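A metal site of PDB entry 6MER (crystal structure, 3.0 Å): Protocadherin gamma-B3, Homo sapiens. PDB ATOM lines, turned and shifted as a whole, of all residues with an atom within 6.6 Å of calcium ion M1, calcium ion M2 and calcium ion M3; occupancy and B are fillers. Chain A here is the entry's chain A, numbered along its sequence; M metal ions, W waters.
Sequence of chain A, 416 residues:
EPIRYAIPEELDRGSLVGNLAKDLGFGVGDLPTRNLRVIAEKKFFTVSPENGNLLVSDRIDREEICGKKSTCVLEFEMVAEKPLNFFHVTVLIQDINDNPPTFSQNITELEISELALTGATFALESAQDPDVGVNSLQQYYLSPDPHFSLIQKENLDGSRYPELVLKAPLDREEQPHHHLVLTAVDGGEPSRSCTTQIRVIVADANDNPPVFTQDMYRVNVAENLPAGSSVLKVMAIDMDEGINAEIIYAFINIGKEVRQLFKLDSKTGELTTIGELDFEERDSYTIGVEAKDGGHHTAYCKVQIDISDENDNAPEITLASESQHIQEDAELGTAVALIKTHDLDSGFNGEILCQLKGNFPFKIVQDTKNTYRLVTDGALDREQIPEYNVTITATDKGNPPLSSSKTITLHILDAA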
ATOM      1  N   GLU A 223       2.690  -4.115  22.309  1.00  0.00           N
ATOM      2  CA  GLU A 223       2.030  -3.439  21.192  1.00  0.00           C
ATOM      3  C   GLU A 223       1.317  -2.165  21.619  1.00  0.00           C
ATOM      4  O   GLU A 223       1.086  -1.290  20.783  1.00  0.00           O
ATOM      5  CB  GLU A 223       1.050  -4.392  20.499  1.00  0.00           C
ATOM      6  CG  GLU A 223       0.054  -5.048  21.431  1.00  0.00           C
ATOM      7  CD  GLU A 223      -0.902  -5.960  20.698  1.00  0.00           C
ATOM      8  OE1 GLU A 223      -1.157  -5.718  19.501  1.00  0.00           O
ATOM      9  OE2 GLU A 223      -1.400  -6.923  21.318  1.00  0.00           O
ATOM     10  N   LEU A 277       2.409   0.190  17.249  1.00  0.00           N
ATOM     11  CA  LEU A 277       2.719  -1.225  17.150  1.00  0.00           C
ATOM     12  C   LEU A 277       1.451  -2.058  17.245  1.00  0.00           C
ATOM     13  O   LEU A 277       0.510  -1.708  17.956  1.00  0.00           O
ATOM     14  CB  LEU A 277       3.704  -1.638  18.255  1.00  0.00           C
ATOM     15  CG  LEU A 277       5.110  -1.029  18.270  1.00  0.00           C
ATOM     16  CD1 LEU A 277       5.681  -0.928  16.853  1.00  0.00           C
ATOM     17  CD2 LEU A 277       5.131   0.329  18.964  1.00  0.00           C
ATOM     18  N   ASP A 278       1.439  -3.178  16.514  1.00  0.00           N
ATOM     19  CA  ASP A 278       0.292  -4.082  16.504  1.00  0.00           C
ATOM     20  C   ASP A 278       0.817  -5.508  16.390  1.00  0.00           C
ATOM     21  O   ASP A 278       1.401  -5.868  15.370  1.00  0.00           O
ATOM     22  CB  ASP A 278      -0.663  -3.749  15.362  1.00  0.00           C
ATOM     23  CG  ASP A 278      -1.983  -4.486  15.481  1.00  0.00           C
ATOM     24  OD1 ASP A 278      -2.738  -4.219  16.433  1.00  0.00           O
ATOM     25  OD2 ASP A 278      -2.270  -5.334  14.612  1.00  0.00           O
ATOM     26  N   PHE A 279       0.607  -6.303  17.449  1.00  0.00           N
ATOM     27  CA  PHE A 279       1.047  -7.689  17.423  1.00  0.00           C
ATOM     28  C   PHE A 279       0.286  -8.509  16.381  1.00  0.00           C
ATOM     29  O   PHE A 279       0.809  -9.502  15.870  1.00  0.00           O
ATOM     30  CB  PHE A 279       0.892  -8.311  18.811  1.00  0.00           C
ATOM     31  CG  PHE A 279       1.367  -9.730  18.905  1.00  0.00           C
ATOM     32  CD1 PHE A 279       2.704 -10.009  19.094  1.00  0.00           C
ATOM     33  CD2 PHE A 279       0.470 -10.783  18.810  1.00  0.00           C
ATOM     34  CE1 PHE A 279       3.150 -11.324  19.189  1.00  0.00           C
ATOM     35  CE2 PHE A 279       0.903 -12.093  18.903  1.00  0.00           C
ATOM     36  CZ  PHE A 279       2.246 -12.355  19.093  1.00  0.00           C
ATOM     37  N   GLU A 280      -0.956  -8.106  16.071  1.00  0.00           N
ATOM     38  CA  GLU A 280      -1.736  -8.831  15.079  1.00  0.00           C
ATOM     39  C   GLU A 280      -1.270  -8.569  13.653  1.00  0.00           C
ATOM     40  O   GLU A 280      -1.518  -9.402  12.773  1.00  0.00           O
ATOM     41  CB  GLU A 280      -3.220  -8.478  15.222  1.00  0.00           C
ATOM     42  CG  GLU A 280      -3.922  -9.160  16.389  1.00  0.00           C
ATOM     43  CD  GLU A 280      -3.413  -8.677  17.741  1.00  0.00           C
ATOM     44  OE1 GLU A 280      -2.939  -7.525  17.828  1.00  0.00           O
ATOM     45  OE2 GLU A 280      -3.500  -9.453  18.714  1.00  0.00           O
ATOM     46  N   GLU A 281      -0.604  -7.440  13.407  1.00  0.00           N
ATOM     47  CA  GLU A 281      -0.110  -7.122  12.078  1.00  0.00           C
ATOM     48  C   GLU A 281       1.296  -7.667  11.858  1.00  0.00           C
ATOM     49  O   GLU A 281       1.562  -8.305  10.831  1.00  0.00           O
ATOM     50  CB  GLU A 281      -0.129  -5.603  11.866  1.00  0.00           C
ATOM     51  CG  GLU A 281       0.349  -5.154  10.485  1.00  0.00           C
ATOM     52  CD  GLU A 281      -0.634  -5.475   9.380  1.00  0.00           C
ATOM     53  OE1 GLU A 281      -1.804  -5.808   9.686  1.00  0.00           O
ATOM     54  OE2 GLU A 281      -0.245  -5.408   8.200  1.00  0.00           O
ATOM     55  N   SER A 308       5.211  -8.031  22.233  1.00  0.00           N
ATOM     56  CA  SER A 308       4.394  -8.900  23.073  1.00  0.00           C
ATOM     57  C   SER A 308       2.914  -8.675  22.789  1.00  0.00           C
ATOM     58  O   SER A 308       2.491  -7.566  22.452  1.00  0.00           O
ATOM     59  CB  SER A 308       4.693  -8.652  24.553  1.00  0.00           C
ATOM     60  OG  SER A 308       6.046  -8.913  24.860  1.00  0.00           O
ATOM     61  N   ASP A 309       2.145  -9.744  22.928  1.00  0.00           N
ATOM     62  CA  ASP A 309       0.709  -9.687  22.672  1.00  0.00           C
ATOM     63  C   ASP A 309      -0.006  -9.083  23.886  1.00  0.00           C
ATOM     64  O   ASP A 309       0.085  -9.626  24.991  1.00  0.00           O
ATOM     65  CB  ASP A 309       0.159 -11.074  22.359  1.00  0.00           C
ATOM     66  CG  ASP A 309      -1.303 -11.062  21.978  1.00  0.00           C
ATOM     67  OD1 ASP A 309      -1.818  -9.978  21.623  1.00  0.00           O
ATOM     68  OD2 ASP A 309      -1.941 -12.132  22.034  1.00  0.00           O
ATOM     69  N   GLU A 310      -0.706  -7.977  23.666  1.00  0.00           N
ATOM     70  CA  GLU A 310      -1.548  -7.371  24.690  1.00  0.00           C
ATOM     71  C   GLU A 310      -3.013  -7.674  24.400  1.00  0.00           C
ATOM     72  O   GLU A 310      -3.419  -7.808  23.245  1.00  0.00           O
ATOM     73  CB  GLU A 310      -1.319  -5.860  24.754  1.00  0.00           C
ATOM     74  CG  GLU A 310      -0.040  -5.448  25.455  1.00  0.00           C
ATOM     75  CD  GLU A 310      -0.091  -5.664  26.950  1.00  0.00           C
ATOM     76  OE1 GLU A 310      -1.199  -5.825  27.501  1.00  0.00           O
ATOM     77  OE2 GLU A 310       0.984  -5.674  27.591  1.00  0.00           O
ATOM     78  N   ASN A 311      -3.804  -7.773  25.463  1.00  0.00           N
ATOM     79  CA  ASN A 311      -5.226  -8.077  25.354  1.00  0.00           C
ATOM     80  C   ASN A 311      -5.996  -6.805  24.994  1.00  0.00           C
ATOM     81  O   ASN A 311      -6.719  -6.219  25.793  1.00  0.00           O
ATOM     82  CB  ASN A 311      -5.748  -8.700  26.634  1.00  0.00           C
ATOM     83  CG  ASN A 311      -7.098  -9.355  26.466  1.00  0.00           C
ATOM     84  OD1 ASN A 311      -7.427  -9.861  25.389  1.00  0.00           O
ATOM     85  ND2 ASN A 311      -7.908  -9.352  27.519  1.00  0.00           N
ATOM     86  N   ASP A 312      -5.821  -6.379  23.743  1.00  0.00           N
ATOM     87  CA  ASP A 312      -6.458  -5.177  23.222  1.00  0.00           C
ATOM     88  C   ASP A 312      -7.549  -5.474  22.210  1.00  0.00           C
ATOM     89  O   ASP A 312      -8.008  -4.565  21.509  1.00  0.00           O
ATOM     90  CB  ASP A 312      -5.407  -4.235  22.614  1.00  0.00           C
ATOM     91  CG  ASP A 312      -4.552  -4.920  21.560  1.00  0.00           C
ATOM     92  OD1 ASP A 312      -4.777  -6.127  21.297  1.00  0.00           O
ATOM     93  OD2 ASP A 312      -3.659  -4.252  21.004  1.00  0.00           O
ATOM     94  N   ASN A 313      -7.979  -6.737  22.099  1.00  0.00           N
ATOM     95  CA  ASN A 313      -9.050  -7.124  21.202  1.00  0.00           C
ATOM     96  C   ASN A 313     -10.089  -7.936  21.983  1.00  0.00           C
ATOM     97  O   ASN A 313      -9.724  -8.888  22.679  1.00  0.00           O
ATOM     98  CB  ASN A 313      -8.524  -7.938  20.015  1.00  0.00           C
ATOM     99  CG  ASN A 313      -7.880  -7.061  18.956  1.00  0.00           C
ATOM    100  OD1 ASN A 313      -8.539  -6.630  18.015  1.00  0.00           O
ATOM    101  ND2 ASN A 313      -6.592  -6.804  19.104  1.00  0.00           N
ATOM    102  N   ALA A 314     -11.347  -7.546  21.858  1.00  0.00           N
ATOM    103  CA  ALA A 314     -12.427  -8.253  22.548  1.00  0.00           C
ATOM    104  C   ALA A 314     -13.008  -9.345  21.653  1.00  0.00           C
ATOM    105  O   ALA A 314     -13.079  -9.176  20.428  1.00  0.00           O
ATOM    106  CB  ALA A 314     -13.534  -7.282  22.945  1.00  0.00           C
ATOM    107  N   PRO A 315     -13.418 -10.473  22.234  1.00  0.00           N
ATOM    108  CA  PRO A 315     -13.998 -11.559  21.431  1.00  0.00           C
ATOM    109  C   PRO A 315     -15.344 -11.136  20.851  1.00  0.00           C
ATOM    110  O   PRO A 315     -16.255 -10.762  21.578  1.00  0.00           O
ATOM    111  CB  PRO A 315     -14.152 -12.705  22.435  1.00  0.00           C
ATOM    112  CG  PRO A 315     -13.271 -12.344  23.596  1.00  0.00           C
ATOM    113  CD  PRO A 315     -13.284 -10.842  23.651  1.00  0.00           C
ATOM    114  N   ASP A 343     -11.050 -14.590  18.720  1.00  0.00           N
ATOM    115  CA  ASP A 343     -10.341 -13.448  19.276  1.00  0.00           C
ATOM    116  C   ASP A 343      -9.038 -13.264  18.510  1.00  0.00           C
ATOM    117  O   ASP A 343      -8.278 -14.229  18.330  1.00  0.00           O
ATOM    118  CB  ASP A 343     -10.070 -13.636  20.763  1.00  0.00           C
ATOM    119  CG  ASP A 343      -9.662 -12.357  21.449  1.00  0.00           C
ATOM    120  OD1 ASP A 343     -10.555 -11.602  21.893  1.00  0.00           O
ATOM    121  OD2 ASP A 343      -8.446 -12.089  21.547  1.00  0.00           O
ATOM    122  N   LEU A 344      -8.781 -12.039  18.049  1.00  0.00           N
ATOM    123  CA  LEU A 344      -7.607 -11.778  17.225  1.00  0.00           C
ATOM    124  C   LEU A 344      -6.300 -11.962  17.997  1.00  0.00           C
ATOM    125  O   LEU A 344      -5.267 -12.212  17.374  1.00  0.00           O
ATOM    126  CB  LEU A 344      -7.673 -10.367  16.652  1.00  0.00           C
ATOM    127  CG  LEU A 344      -8.898 -10.041  15.790  1.00  0.00           C
ATOM    128  CD1 LEU A 344      -8.773  -8.650  15.186  1.00  0.00           C
ATOM    129  CD2 LEU A 344      -9.091 -11.098  14.708  1.00  0.00           C
ATOM    130  N   ASP A 345      -6.333 -11.861  19.319  1.00  0.00           N
ATOM    131  CA  ASP A 345      -5.130 -12.028  20.106  1.00  0.00           C
ATOM    132  C   ASP A 345      -4.713 -13.500  20.144  1.00  0.00           C
ATOM    133  O   ASP A 345      -5.498 -14.409  19.836  1.00  0.00           O
ATOM    134  CB  ASP A 345      -5.335 -11.518  21.532  1.00  0.00           C
ATOM    135  CG  ASP A 345      -5.934 -10.137  21.574  1.00  0.00           C
ATOM    136  OD1 ASP A 345      -5.621  -9.322  20.672  1.00  0.00           O
ATOM    137  OD2 ASP A 345      -6.721  -9.844  22.503  1.00  0.00           O
ATOM    138  N   SER A 346      -3.457 -13.728  20.504  1.00  0.00           N
ATOM    139  CA  SER A 346      -2.897 -15.070  20.594  1.00  0.00           C
ATOM    140  C   SER A 346      -2.772 -15.499  22.058  1.00  0.00           C
ATOM    141  O   SER A 346      -3.027 -14.722  22.989  1.00  0.00           O
ATOM    142  CB  SER A 346      -1.536 -15.133  19.901  1.00  0.00           C
ATOM    143  OG  SER A 346      -1.637 -14.752  18.543  1.00  0.00           O
ATOM    144  N   PHE A 348      -3.435 -17.210  25.658  1.00  0.00           N
ATOM    145  CA  PHE A 348      -4.642 -17.222  26.483  1.00  0.00           C
ATOM    146  C   PHE A 348      -5.493 -15.974  26.260  1.00  0.00           C
ATOM    147  O   PHE A 348      -6.674 -15.980  26.625  1.00  0.00           O
ATOM    148  CB  PHE A 348      -4.276 -17.349  27.961  1.00  0.00           C
ATOM    149  CG  PHE A 348      -3.963 -18.750  28.384  1.00  0.00           C
ATOM    150  CD1 PHE A 348      -4.980 -19.623  28.749  1.00  0.00           C
ATOM    151  CD2 PHE A 348      -2.656 -19.214  28.421  1.00  0.00           C
ATOM    152  CE1 PHE A 348      -4.709 -20.914  29.133  1.00  0.00           C
ATOM    153  CE2 PHE A 348      -2.372 -20.511  28.808  1.00  0.00           C
ATOM    154  CZ  PHE A 348      -3.396 -21.362  29.171  1.00  0.00           C
ATOM    155  N   ASN A 349      -4.919 -14.918  25.681  1.00  0.00           N
ATOM    156  CA  ASN A 349      -5.726 -13.755  25.325  1.00  0.00           C
ATOM    157  C   ASN A 349      -6.707 -14.058  24.206  1.00  0.00           C
ATOM    158  O   ASN A 349      -7.670 -13.307  24.017  1.00  0.00           O
ATOM    159  CB  ASN A 349      -4.815 -12.598  24.902  1.00  0.00           C
ATOM    160  CG  ASN A 349      -3.810 -12.217  25.978  1.00  0.00           C
ATOM    161  OD1 ASN A 349      -4.144 -12.163  27.156  1.00  0.00           O
ATOM    162  ND2 ASN A 349      -2.576 -11.965  25.563  1.00  0.00           N
ATOM    163  N   GLY A 350      -6.500 -15.153  23.472  1.00  0.00           N
ATOM    164  CA  GLY A 350      -7.368 -15.513  22.367  1.00  0.00           C
ATOM    165  C   GLY A 350      -8.361 -16.606  22.707  1.00  0.00           C
ATOM    166  O   GLY A 350      -9.377 -16.756  22.029  1.00  0.00           O
ATOM    167  N   GLU A 351      -8.089 -17.376  23.762  1.00  0.00           N
ATOM    168  CA  GLU A 351      -9.023 -18.394  24.198  1.00  0.00           C
ATOM    169  C   GLU A 351     -10.278 -17.750  24.780  1.00  0.00           C
ATOM    170  O   GLU A 351     -10.194 -16.796  25.553  1.00  0.00           O
ATOM    171  CB  GLU A 351      -8.380 -19.329  25.224  1.00  0.00           C
ATOM    172  CG  GLU A 351      -7.293 -20.222  24.641  1.00  0.00           C
ATOM    173  CD  GLU A 351      -6.882 -21.325  25.601  1.00  0.00           C
ATOM    174  OE1 GLU A 351      -7.497 -21.444  26.676  1.00  0.00           O
ATOM    175  OE2 GLU A 351      -5.946 -22.093  25.268  1.00  0.00           O
ATOM    176  N   ASP A 396     -12.807 -13.603  27.170  1.00  0.00           N
ATOM    177  CA  ASP A 396     -11.503 -14.225  26.959  1.00  0.00           C
ATOM    178  C   ASP A 396     -10.829 -14.516  28.293  1.00  0.00           C
ATOM    179  O   ASP A 396     -11.297 -14.116  29.363  1.00  0.00           O
ATOM    180  CB  ASP A 396     -10.631 -13.334  26.081  1.00  0.00           C
ATOM    181  CG  ASP A 396     -10.479 -11.914  26.618  1.00  0.00           C
ATOM    182  OD1 ASP A 396     -10.850 -11.670  27.783  1.00  0.00           O
ATOM    183  OD2 ASP A 396     -10.005 -11.052  25.864  1.00  0.00           O
ATOM    184  N   LYS A 397      -9.705 -15.236  28.220  1.00  0.00           N
ATOM    185  CA  LYS A 397      -8.960 -15.629  29.410  1.00  0.00           C
ATOM    186  C   LYS A 397      -7.699 -14.796  29.612  1.00  0.00           C
ATOM    187  O   LYS A 397      -6.729 -15.262  30.216  1.00  0.00           O
ATOM    188  CB  LYS A 397      -8.596 -17.115  29.327  1.00  0.00           C
ATOM    189  CG  LYS A 397      -9.813 -18.028  29.219  1.00  0.00           C
ATOM    190  CD  LYS A 397      -9.390 -19.488  29.128  1.00  0.00           C
ATOM    191  CE  LYS A 397     -10.604 -20.396  29.012  1.00  0.00           C
ATOM    192  NZ  LYS A 397     -10.208 -21.833  28.949  1.00  0.00           N
ATOM    193  N   GLY A 398      -7.691 -13.559  29.101  1.00  0.00           N
ATOM    194  CA  GLY A 398      -6.547 -12.685  29.229  1.00  0.00           C
ATOM    195  C   GLY A 398      -6.541 -11.903  30.524  1.00  0.00           C
ATOM    196  O   GLY A 398      -7.330 -12.144  31.437  1.00  0.00           O
ATOM    197  N   LEU A 402     -11.440  -9.250  28.643  1.00  0.00           N
ATOM    198  CA  LEU A 402     -12.426  -8.479  27.907  1.00  0.00           C
ATOM    199  C   LEU A 402     -13.561  -9.403  27.452  1.00  0.00           C
ATOM    200  O   LEU A 402     -13.377 -10.612  27.313  1.00  0.00           O
ATOM    201  CB  LEU A 402     -11.809  -7.782  26.688  1.00  0.00           C
ATOM    202  CG  LEU A 402     -10.702  -6.771  26.984  1.00  0.00           C
ATOM    203  CD1 LEU A 402     -10.162  -6.167  25.687  1.00  0.00           C
ATOM    204  CD2 LEU A 402     -11.211  -5.669  27.905  1.00  0.00           C
HETATM  205 CA    CA M   1      -3.500  -5.208  18.648  1.00  0.00          CA
HETATM  206 CA    CA M   2      -3.433  -8.167  20.770  1.00  0.00          CA
HETATM  207 CA    CA M   3      -8.811 -10.936  23.648  1.00  0.00          CA
HETATM  208  O   HOH W   1      -6.408  -3.592  18.607  1.00  0.00           O
HETATM  209  O   HOH W   2      -2.649  -2.795  18.795  1.00  0.00           O
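OD1 of Asp 312 lies close to ND2 of Asn 313. The side-chain carboxylate (OE1) of Glu 223 lies close to the backbone NH (N) of Phe 279 (2.8 Å). The backbone NH (N) of Glu 223 lies within hydrogen-bond range of the backbone carbonyl oxygen (O) of Ser 308 (3.5 Å). OD1 of Asp 396 lies within hydrogen-bond range of N of Leu 402, 2.6 Å away. The side-chain carboxylate of Asp 278 sits at hydrogen-bond distance from the backbone NH of Glu 281, 2.9 Å away. OD2 of Asp 309 is in hydrogen-bond range of N of Ser 346 (2.7 Å).
Calcium ion M1 is bound by OE1 of Glu 280 (2.5 Å). The side-chain carboxylate (OD1) of Asp 278 is bound to calcium ion M1, 2.5 Å away. Calcium ion M1 is bound by OE1 of Glu 223 (2.5 Å). OD2 of Asp 312 is bound to calcium ion M1. Water W2 binds calcium ion M1, at 2.6 Å. Slightly farther from calcium ion M1 lies the side-chain carboxylate (OD1) of Asp 312 (3.1 Å).
Water W1 bridges the side-chain amide nitrogen of Asn 313 (3.3 Å) and the backbone carbonyl oxygen of Asp 312 (3.5 Å).
Calcium ion M3 is bound by OD2 of Asp 343 (2.4 Å). O of Asn 313 binds calcium ion M3 (2.4 Å). OD1 of Asn 311 is bound to calcium ion M3. Calcium ion M3 is bound by the side-chain carboxylate (OD2) of Asp 396 (2.5 Å). The side-chain carboxylate (OD1) of Asp 343 binds calcium ion M3. The side-chain carboxylate (OD2) of Asp 345 binds calcium ion M3. The backbone carbonyl oxygen (O) of Asn 349 is bound to calcium ion M3 (2.7 Å). Calcium ion M3 has seven donor atoms within binding distance.
Of the 26 residues printed, 5 come within 4 Å of calcium ion M1.
Six residues have an atom within 4 Å of calcium ion M3: Asn 311, Asn 313, Asp 343, Asp 345, Asn 349 and Asp 396. The nearest printed residue that does not touch calcium ion M3 is Pro 315 (4.5 Å).
OE2 of Glu 280 is bound to calcium ion M2 (2.4 Å). OE2 of Glu 223 binds calcium ion M2 (2.4 Å). Calcium ion M2 is bound by OD1 of Asp 345 (2.5 Å). The side-chain carboxylate (OD1) of Asp 312 is bound to calcium ion M2 (2.5 Å). Calcium ion M2 is bound by O of Glu 310, at 2.5 Å. The side-chain carboxylate (OD1) of Asp 309 binds calcium ion M2. Slightly farther from calcium ion M2 lies OE1 of Glu 280 (3.1 Å).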
